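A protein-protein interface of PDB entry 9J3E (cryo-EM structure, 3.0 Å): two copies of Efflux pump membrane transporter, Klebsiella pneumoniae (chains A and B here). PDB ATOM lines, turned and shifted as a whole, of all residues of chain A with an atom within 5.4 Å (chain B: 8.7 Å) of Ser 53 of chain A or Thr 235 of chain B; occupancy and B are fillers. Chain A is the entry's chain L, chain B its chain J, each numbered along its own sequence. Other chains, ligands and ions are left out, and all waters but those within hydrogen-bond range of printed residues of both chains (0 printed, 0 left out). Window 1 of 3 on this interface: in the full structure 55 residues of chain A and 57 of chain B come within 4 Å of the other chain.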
ATOM      1  N   GLY A  51     -12.337  -5.621 -20.156  1.00  0.00           N
ATOM      2  CA  GLY A  51     -10.983  -5.288 -20.521  1.00  0.00           C
ATOM      3  C   GLY A  51     -10.567  -5.686 -21.917  1.00  0.00           C
ATOM      4  O   GLY A  51      -9.370  -5.630 -22.224  1.00  0.00           O
ATOM      5  N   ALA A  52     -11.495  -6.096 -22.771  1.00  0.00           N
ATOM      6  CA  ALA A  52     -11.168  -6.396 -24.154  1.00  0.00           C
ATOM      7  C   ALA A  52     -11.392  -5.164 -25.014  1.00  0.00           C
ATOM      8  O   ALA A  52     -12.386  -4.453 -24.854  1.00  0.00           O
ATOM      9  CB  ALA A  52     -12.004  -7.563 -24.672  1.00  0.00           C
ATOM     10  N   SER A  53     -10.458  -4.913 -25.924  1.00  0.00           N
ATOM     11  CA  SER A  53     -10.524  -3.732 -26.764  1.00  0.00           C
ATOM     12  C   SER A  53     -11.712  -3.813 -27.720  1.00  0.00           C
ATOM     13  O   SER A  53     -12.422  -4.817 -27.797  1.00  0.00           O
ATOM     14  CB  SER A  53      -9.230  -3.566 -27.557  1.00  0.00           C
ATOM     15  OG  SER A  53      -9.166  -4.495 -28.625  1.00  0.00           O
ATOM     16  N   ALA A  54     -11.928  -2.722 -28.453  1.00  0.00           N
ATOM     17  CA  ALA A  54     -13.026  -2.691 -29.410  1.00  0.00           C
ATOM     18  C   ALA A  54     -12.819  -3.708 -30.519  1.00  0.00           C
ATOM     19  O   ALA A  54     -13.731  -4.471 -30.852  1.00  0.00           O
ATOM     20  CB  ALA A  54     -13.165  -1.290 -29.997  1.00  0.00           C
ATOM     21  N   GLN A  55     -11.623  -3.745 -31.098  1.00  0.00           N
ATOM     22  CA  GLN A  55     -11.379  -4.671 -32.192  1.00  0.00           C
ATOM     23  C   GLN A  55     -11.390  -6.109 -31.704  1.00  0.00           C
ATOM     24  O   GLN A  55     -11.888  -7.001 -32.401  1.00  0.00           O
ATOM     25  CB  GLN A  55     -10.054  -4.348 -32.870  1.00  0.00           C
ATOM     26  CG  GLN A  55      -9.803  -5.139 -34.139  1.00  0.00           C
ATOM     27  CD  GLN A  55     -11.055  -5.334 -34.966  1.00  0.00           C
ATOM     28  OE1 GLN A  55     -11.428  -4.470 -35.756  1.00  0.00           O
ATOM     29  NE2 GLN A  55     -11.697  -6.483 -34.806  1.00  0.00           N
ATOM     30  N   VAL A  56     -10.838  -6.355 -30.517  1.00  0.00           N
ATOM     31  CA  VAL A  56     -10.814  -7.710 -29.977  1.00  0.00           C
ATOM     32  C   VAL A  56     -12.231  -8.219 -29.769  1.00  0.00           C
ATOM     33  O   VAL A  56     -12.578  -9.332 -30.178  1.00  0.00           O
ATOM     34  CB  VAL A  56     -10.003  -7.752 -28.672  1.00  0.00           C
ATOM     35  CG1 VAL A  56     -10.276  -9.037 -27.923  1.00  0.00           C
ATOM     36  CG2 VAL A  56      -8.528  -7.614 -28.973  1.00  0.00           C
ATOM     37  N   LEU A  57     -13.078  -7.402 -29.147  1.00  0.00           N
ATOM     38  CA  LEU A  57     -14.463  -7.799 -28.936  1.00  0.00           C
ATOM     39  C   LEU A  57     -15.200  -7.949 -30.258  1.00  0.00           C
ATOM     40  O   LEU A  57     -16.086  -8.798 -30.392  1.00  0.00           O
ATOM     41  CB  LEU A  57     -15.164  -6.778 -28.048  1.00  0.00           C
ATOM     42  CG  LEU A  57     -16.499  -7.229 -27.482  1.00  0.00           C
ATOM     43  CD1 LEU A  57     -16.387  -8.656 -27.051  1.00  0.00           C
ATOM     44  CD2 LEU A  57     -16.885  -6.361 -26.318  1.00  0.00           C
ATOM     45  N   THR A  58     -14.851  -7.123 -31.244  1.00  0.00           N
ATOM     46  CA  THR A  58     -15.487  -7.219 -32.551  1.00  0.00           C
ATOM     47  C   THR A  58     -15.200  -8.558 -33.204  1.00  0.00           C
ATOM     48  O   THR A  58     -16.114  -9.255 -33.653  1.00  0.00           O
ATOM     49  CB  THR A  58     -15.001  -6.095 -33.456  1.00  0.00           C
ATOM     50  OG1 THR A  58     -15.539  -4.851 -33.008  1.00  0.00           O
ATOM     51  CG2 THR A  58     -15.435  -6.351 -34.878  1.00  0.00           C
ATOM     52  N   ASN A  83     -17.582  -1.328 -28.229  1.00  0.00           N
ATOM     53  CA  ASN A  83     -16.899  -0.211 -27.601  1.00  0.00           C
ATOM     54  C   ASN A  83     -15.744  -0.698 -26.739  1.00  0.00           C
ATOM     55  O   ASN A  83     -15.699  -1.854 -26.311  1.00  0.00           O
ATOM     56  CB  ASN A  83     -17.864   0.620 -26.757  1.00  0.00           C
ATOM     57  CG  ASN A  83     -19.102   1.018 -27.516  1.00  0.00           C
ATOM     58  OD1 ASN A  83     -20.194   0.522 -27.249  1.00  0.00           O
ATOM     59  ND2 ASN A  83     -18.942   1.924 -28.467  1.00  0.00           N
ATOM     60  N   ALA A  84     -14.809   0.216 -26.479  1.00  0.00           N
ATOM     61  CA  ALA A  84     -13.617  -0.124 -25.714  1.00  0.00           C
ATOM     62  C   ALA A  84     -13.930  -0.482 -24.273  1.00  0.00           C
ATOM     63  O   ALA A  84     -13.064  -1.026 -23.581  1.00  0.00           O
ATOM     64  CB  ALA A  84     -12.623   1.033 -25.742  1.00  0.00           C
ATOM     65  N   PRO A 721      -5.961   7.390 -29.512  1.00  0.00           N
ATOM     66  CA  PRO A 721      -4.608   6.836 -29.448  1.00  0.00           C
ATOM     67  C   PRO A 721      -4.592   5.572 -28.607  1.00  0.00           C
ATOM     68  O   PRO A 721      -5.300   5.462 -27.606  1.00  0.00           O
ATOM     69  CB  PRO A 721      -3.795   7.960 -28.801  1.00  0.00           C
ATOM     70  CG  PRO A 721      -4.577   9.192 -29.075  1.00  0.00           C
ATOM     71  CD  PRO A 721      -6.009   8.779 -29.035  1.00  0.00           C
ATOM     72  N   GLN A 722      -3.780   4.608 -29.026  1.00  0.00           N
ATOM     73  CA  GLN A 722      -3.672   3.331 -28.343  1.00  0.00           C
ATOM     74  C   GLN A 722      -2.233   3.085 -27.933  1.00  0.00           C
ATOM     75  O   GLN A 722      -1.302   3.639 -28.518  1.00  0.00           O
ATOM     76  CB  GLN A 722      -4.141   2.182 -29.215  1.00  0.00           C
ATOM     77  CG  GLN A 722      -5.602   2.225 -29.537  1.00  0.00           C
ATOM     78  CD  GLN A 722      -6.050   0.984 -30.253  1.00  0.00           C
ATOM     79  OE1 GLN A 722      -5.233   0.154 -30.648  1.00  0.00           O
ATOM     80  NE2 GLN A 722      -7.357   0.829 -30.400  1.00  0.00           N
ATOM     81  N   LEU A 723      -2.058   2.241 -26.926  1.00  0.00           N
ATOM     82  CA  LEU A 723      -0.737   1.895 -26.422  1.00  0.00           C
ATOM     83  C   LEU A 723      -0.478   0.422 -26.718  1.00  0.00           C
ATOM     84  O   LEU A 723      -0.697  -0.439 -25.870  1.00  0.00           O
ATOM     85  CB  LEU A 723      -0.636   2.179 -24.938  1.00  0.00           C
ATOM     86  CG  LEU A 723       0.760   1.975 -24.365  1.00  0.00           C
ATOM     87  CD1 LEU A 723       1.680   2.964 -25.015  1.00  0.00           C
ATOM     88  CD2 LEU A 723       0.753   2.163 -22.867  1.00  0.00           C
ATOM     89  N   ARG A 724       0.008   0.137 -27.919  1.00  0.00           N
ATOM     90  CA  ARG A 724       0.381  -1.228 -28.252  1.00  0.00           C
ATOM     91  C   ARG A 724       1.565  -1.660 -27.400  1.00  0.00           C
ATOM     92  O   ARG A 724       2.505  -0.892 -27.185  1.00  0.00           O
ATOM     93  CB  ARG A 724       0.725  -1.333 -29.738  1.00  0.00           C
ATOM     94  CG  ARG A 724       1.870  -2.268 -30.056  1.00  0.00           C
ATOM     95  CD  ARG A 724       1.415  -3.705 -30.142  1.00  0.00           C
ATOM     96  NE  ARG A 724       0.126  -3.829 -30.806  1.00  0.00           N
ATOM     97  CZ  ARG A 724      -0.057  -3.698 -32.111  1.00  0.00           C
ATOM     98  NH1 ARG A 724       0.954  -3.461 -32.929  1.00  0.00           N
ATOM     99  NH2 ARG A 724      -1.284  -3.816 -32.608  1.00  0.00           N
ATOM    100  N   GLN B 215      -5.856 -14.686 -27.573  1.00  0.00           N
ATOM    101  CA  GLN B 215      -6.103 -13.256 -27.517  1.00  0.00           C
ATOM    102  C   GLN B 215      -5.985 -12.741 -26.089  1.00  0.00           C
ATOM    103  O   GLN B 215      -6.277 -13.446 -25.122  1.00  0.00           O
ATOM    104  CB  GLN B 215      -7.443 -12.948 -28.209  1.00  0.00           C
ATOM    105  CG  GLN B 215      -8.774 -13.552 -27.687  1.00  0.00           C
ATOM    106  CD  GLN B 215      -9.165 -13.336 -26.236  1.00  0.00           C
ATOM    107  OE1 GLN B 215      -8.621 -12.498 -25.531  1.00  0.00           O
ATOM    108  NE2 GLN B 215     -10.130 -14.127 -25.783  1.00  0.00           N
ATOM    109  N   VAL B 216      -5.499 -11.512 -25.964  1.00  0.00           N
ATOM    110  CA  VAL B 216      -5.122 -10.941 -24.675  1.00  0.00           C
ATOM    111  C   VAL B 216      -6.029  -9.760 -24.355  1.00  0.00           C
ATOM    112  O   VAL B 216      -5.880  -8.688 -24.956  1.00  0.00           O
ATOM    113  CB  VAL B 216      -3.648 -10.513 -24.678  1.00  0.00           C
ATOM    114  CG1 VAL B 216      -3.336  -9.678 -23.457  1.00  0.00           C
ATOM    115  CG2 VAL B 216      -2.746 -11.722 -24.745  1.00  0.00           C
ATOM    116  N   PRO B 217      -6.965  -9.895 -23.426  1.00  0.00           N
ATOM    117  CA  PRO B 217      -7.837  -8.762 -23.071  1.00  0.00           C
ATOM    118  C   PRO B 217      -7.143  -7.828 -22.087  1.00  0.00           C
ATOM    119  O   PRO B 217      -7.432  -7.782 -20.897  1.00  0.00           O
ATOM    120  CB  PRO B 217      -9.048  -9.456 -22.447  1.00  0.00           C
ATOM    121  CG  PRO B 217      -8.477 -10.668 -21.825  1.00  0.00           C
ATOM    122  CD  PRO B 217      -7.295 -11.102 -22.655  1.00  0.00           C
ATOM    123  N   ALA B 218      -6.198  -7.051 -22.611  1.00  0.00           N
ATOM    124  CA  ALA B 218      -5.306  -6.280 -21.754  1.00  0.00           C
ATOM    125  C   ALA B 218      -6.066  -5.220 -20.972  1.00  0.00           C
ATOM    126  O   ALA B 218      -6.045  -5.209 -19.737  1.00  0.00           O
ATOM    127  CB  ALA B 218      -4.206  -5.644 -22.595  1.00  0.00           C
ATOM    128  N   GLY B 219      -6.744  -4.314 -21.674  1.00  0.00           N
ATOM    129  CA  GLY B 219      -7.485  -3.247 -21.041  1.00  0.00           C
ATOM    130  C   GLY B 219      -6.928  -1.886 -21.411  1.00  0.00           C
ATOM    131  O   GLY B 219      -6.331  -1.709 -22.478  1.00  0.00           O
ATOM    132  N   ALA B 220      -7.128  -0.927 -20.518  1.00  0.00           N
ATOM    133  CA  ALA B 220      -6.709   0.437 -20.782  1.00  0.00           C
ATOM    134  C   ALA B 220      -6.315   1.099 -19.476  1.00  0.00           C
ATOM    135  O   ALA B 220      -7.057   1.029 -18.493  1.00  0.00           O
ATOM    136  CB  ALA B 220      -7.828   1.228 -21.460  1.00  0.00           C
ATOM    137  N   PHE B 221      -5.153   1.743 -19.468  1.00  0.00           N
ATOM    138  CA  PHE B 221      -4.728   2.457 -18.279  1.00  0.00           C
ATOM    139  C   PHE B 221      -5.588   3.696 -18.088  1.00  0.00           C
ATOM    140  O   PHE B 221      -6.206   4.200 -19.024  1.00  0.00           O
ATOM    141  CB  PHE B 221      -3.251   2.831 -18.363  1.00  0.00           C
ATOM    142  CG  PHE B 221      -2.954   3.951 -19.314  1.00  0.00           C
ATOM    143  CD1 PHE B 221      -2.903   5.257 -18.877  1.00  0.00           C
ATOM    144  CD2 PHE B 221      -2.688   3.692 -20.642  1.00  0.00           C
ATOM    145  CE1 PHE B 221      -2.619   6.278 -19.752  1.00  0.00           C
ATOM    146  CE2 PHE B 221      -2.403   4.716 -21.517  1.00  0.00           C
ATOM    147  CZ  PHE B 221      -2.368   6.007 -21.068  1.00  0.00           C
ATOM    148  N   GLY B 222      -5.646   4.172 -16.850  1.00  0.00           N
ATOM    149  CA  GLY B 222      -6.511   5.293 -16.555  1.00  0.00           C
ATOM    150  C   GLY B 222      -7.981   4.963 -16.561  1.00  0.00           C
ATOM    151  O   GLY B 222      -8.808   5.860 -16.723  1.00  0.00           O
ATOM    152  N   SER B 223      -8.332   3.696 -16.382  1.00  0.00           N
ATOM    153  CA  SER B 223      -9.718   3.273 -16.460  1.00  0.00           C
ATOM    154  C   SER B 223     -10.460   3.595 -15.168  1.00  0.00           C
ATOM    155  O   SER B 223      -9.864   3.916 -14.138  1.00  0.00           O
ATOM    156  CB  SER B 223      -9.804   1.775 -16.748  1.00  0.00           C
ATOM    157  OG  SER B 223      -9.564   1.498 -18.115  1.00  0.00           O
ATOM    158  N   LEU B 232      -5.961  10.721 -19.363  1.00  0.00           N
ATOM    159  CA  LEU B 232      -5.758  10.169 -20.707  1.00  0.00           C
ATOM    160  C   LEU B 232      -5.822   8.648 -20.743  1.00  0.00           C
ATOM    161  O   LEU B 232      -4.857   7.981 -21.115  1.00  0.00           O
ATOM    162  CB  LEU B 232      -4.467  10.630 -21.366  1.00  0.00           C
ATOM    163  CG  LEU B 232      -4.580  11.970 -22.089  1.00  0.00           C
ATOM    164  CD1 LEU B 232      -5.834  12.004 -22.980  1.00  0.00           C
ATOM    165  CD2 LEU B 232      -4.503  13.155 -21.170  1.00  0.00           C
ATOM    166  N   THR B 233      -6.939   8.074 -20.313  1.00  0.00           N
ATOM    167  CA  THR B 233      -7.195   6.666 -20.601  1.00  0.00           C
ATOM    168  C   THR B 233      -6.902   6.347 -22.064  1.00  0.00           C
ATOM    169  O   THR B 233      -7.150   7.166 -22.951  1.00  0.00           O
ATOM    170  CB  THR B 233      -8.645   6.316 -20.285  1.00  0.00           C
ATOM    171  OG1 THR B 233      -8.955   5.032 -20.838  1.00  0.00           O
ATOM    172  CG2 THR B 233      -9.572   7.351 -20.880  1.00  0.00           C
ATOM    173  N   ALA B 234      -6.341   5.164 -22.313  1.00  0.00           N
ATOM    174  CA  ALA B 234      -6.070   4.715 -23.670  1.00  0.00           C
ATOM    175  C   ALA B 234      -5.869   3.208 -23.667  1.00  0.00           C
ATOM    176  O   ALA B 234      -5.374   2.641 -22.694  1.00  0.00           O
ATOM    177  CB  ALA B 234      -4.846   5.411 -24.261  1.00  0.00           C
ATOM    178  N   THR B 235      -6.228   2.574 -24.777  1.00  0.00           N
ATOM    179  CA  THR B 235      -6.251   1.123 -24.887  1.00  0.00           C
ATOM    180  C   THR B 235      -4.829   0.557 -24.916  1.00  0.00           C
ATOM    181  O   THR B 235      -3.871   1.241 -25.281  1.00  0.00           O
ATOM    182  CB  THR B 235      -7.053   0.726 -26.134  1.00  0.00           C
ATOM    183  OG1 THR B 235      -8.451   0.764 -25.826  1.00  0.00           O
ATOM    184  CG2 THR B 235      -6.707  -0.659 -26.643  1.00  0.00           C
ATOM    185  N   LEU B 236      -4.694  -0.703 -24.480  1.00  0.00           N
ATOM    186  CA  LEU B 236      -3.408  -1.389 -24.416  1.00  0.00           C
ATOM    187  C   LEU B 236      -3.155  -2.384 -25.545  1.00  0.00           C
ATOM    188  O   LEU B 236      -1.997  -2.718 -25.792  1.00  0.00           O
ATOM    189  CB  LEU B 236      -3.261  -2.115 -23.078  1.00  0.00           C
ATOM    190  CG  LEU B 236      -3.206  -1.184 -21.871  1.00  0.00           C
ATOM    191  CD1 LEU B 236      -2.793  -1.951 -20.642  1.00  0.00           C
ATOM    192  CD2 LEU B 236      -2.264  -0.027 -22.127  1.00  0.00           C
ATOM    193  N   THR B 237      -4.195  -2.897 -26.195  1.00  0.00           N
ATOM    194  CA  THR B 237      -4.119  -3.603 -27.484  1.00  0.00           C
ATOM    195  C   THR B 237      -2.861  -4.464 -27.650  1.00  0.00           C
ATOM    196  O   THR B 237      -2.071  -4.302 -28.579  1.00  0.00           O
ATOM    197  CB  THR B 237      -4.266  -2.630 -28.658  1.00  0.00           C
ATOM    198  OG1 THR B 237      -4.171  -3.357 -29.889  1.00  0.00           O
ATOM    199  CG2 THR B 237      -3.215  -1.530 -28.639  1.00  0.00           C
ATOM    200  N   VAL B 238      -2.702  -5.421 -26.740  1.00  0.00           N
ATOM    201  CA  VAL B 238      -1.663  -6.431 -26.896  1.00  0.00           C
ATOM    202  C   VAL B 238      -2.012  -7.360 -28.050  1.00  0.00           C
ATOM    203  O   VAL B 238      -3.180  -7.720 -28.250  1.00  0.00           O
ATOM    204  CB  VAL B 238      -1.494  -7.222 -25.589  1.00  0.00           C
ATOM    205  CG1 VAL B 238      -0.456  -8.306 -25.756  1.00  0.00           C
ATOM    206  CG2 VAL B 238      -1.115  -6.292 -24.469  1.00  0.00           C
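O of Leu 236 of chain B sits close to O of Leu 723 of chain A, 2.6 Å away. The backbone carbonyl oxygen of Thr 237 of chain B lies within hydrogen-bond range of the guanidinium group of Arg 724 of chain A (3.2 Å). The backbone NH (N) of Gly 219 of chain B lies within hydrogen-bond range of the backbone carbonyl oxygen (O) of Gly 51 of chain A (3.0 Å). O of Gly 51 of chain A sits close to O of Pro 217 of chain B, at 3.2 Å. The backbone carbonyl oxygen (O) of Gly 51 of chain A lies within hydrogen-bond range of the backbone NH (N) of Ala 218 of chain B, at 3.5 Å. O of Thr 235 of chain B sits at hydrogen-bond distance from N of Leu 723 of chain A.
The side-chain hydroxyl (OG) of Ser 53 of chain A is in hydrogen-bond range of the backbone NH (N) of Val 56 of chain A, 3.1 Å away. The backbone NH (N) of Leu 236 of chain B sits at hydrogen-bond distance from the backbone carbonyl oxygen (O) of Gly 219 of chain B, at 2.8 Å. The backbone NH of Phe 221 of chain B is in hydrogen-bond range of the backbone carbonyl oxygen of Ala 234 of chain B (3.4 Å).
Ser 53 of chain A touches Thr 235 of chain B. O of Pro 721 of chain A touches CB of Ala 234 of chain B, at 3.4 Å. Thr 235 of chain B touches Gln 722 of chain A. OE1 of Gln 722 of chain A touches CG2 of Thr 237 of chain B (3.3 Å). Thr 237 of chain B touches Leu 723 of chain A (CG2 to C, 3.9 Å). Arg 724 of chain A touches Leu 236 of chain B (CA to O, 3.7 Å).
Of chain B, only Thr 235 (3.96 Å) comes within 4 Å of Ser 53 of chain A. Thr 235 of chain B touches just these residues of chain A: Ser 53, Gln 722 and Leu 723. No residue of chain B comes within 4 Å of Ala 52 of chain A. No residue of chain B comes within 4 Å of Ala 54 of chain A. Of the printed residues of chain A, Gly 219 of chain B touches Gly 51 (3.0 Å). Of the printed residues of chain A, Thr 237 of chain B touches Gln 722, Leu 723 and Arg 724. The nearest residue of chain B that does not touch Ser 53 of chain A is Thr 237 of chain B (5.1 Å). The nearest residue of chain A that does not touch Thr 235 of chain B is Pro 721 of chain A (4.1 Å). The nearest printed residue of chain B that does not touch Arg 724 of chain A is Thr 235 of chain B (4.8 Å).
Of the 14 printed residues of chain A, 6 touch a printed residue of chain B. Of the 16 printed residues of chain B, 7 touch a printed residue of chain A. Hydrophobic or aromatic side chains of chain B within 4 Å of the printed part of chain A: Pro 217, Ala 234 and Leu 236. Among the printed residues, 12 pairs touch across the chains. Among the printed residues, no Asp or Glu carboxylate lies within 4 Å of a Lys or Arg side-chain nitrogen of the other chain.
No position is printed for both chains. Of the 12 pairs that touch across the chains among the printed residues, none has its exchanged pair printed and touching as well.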
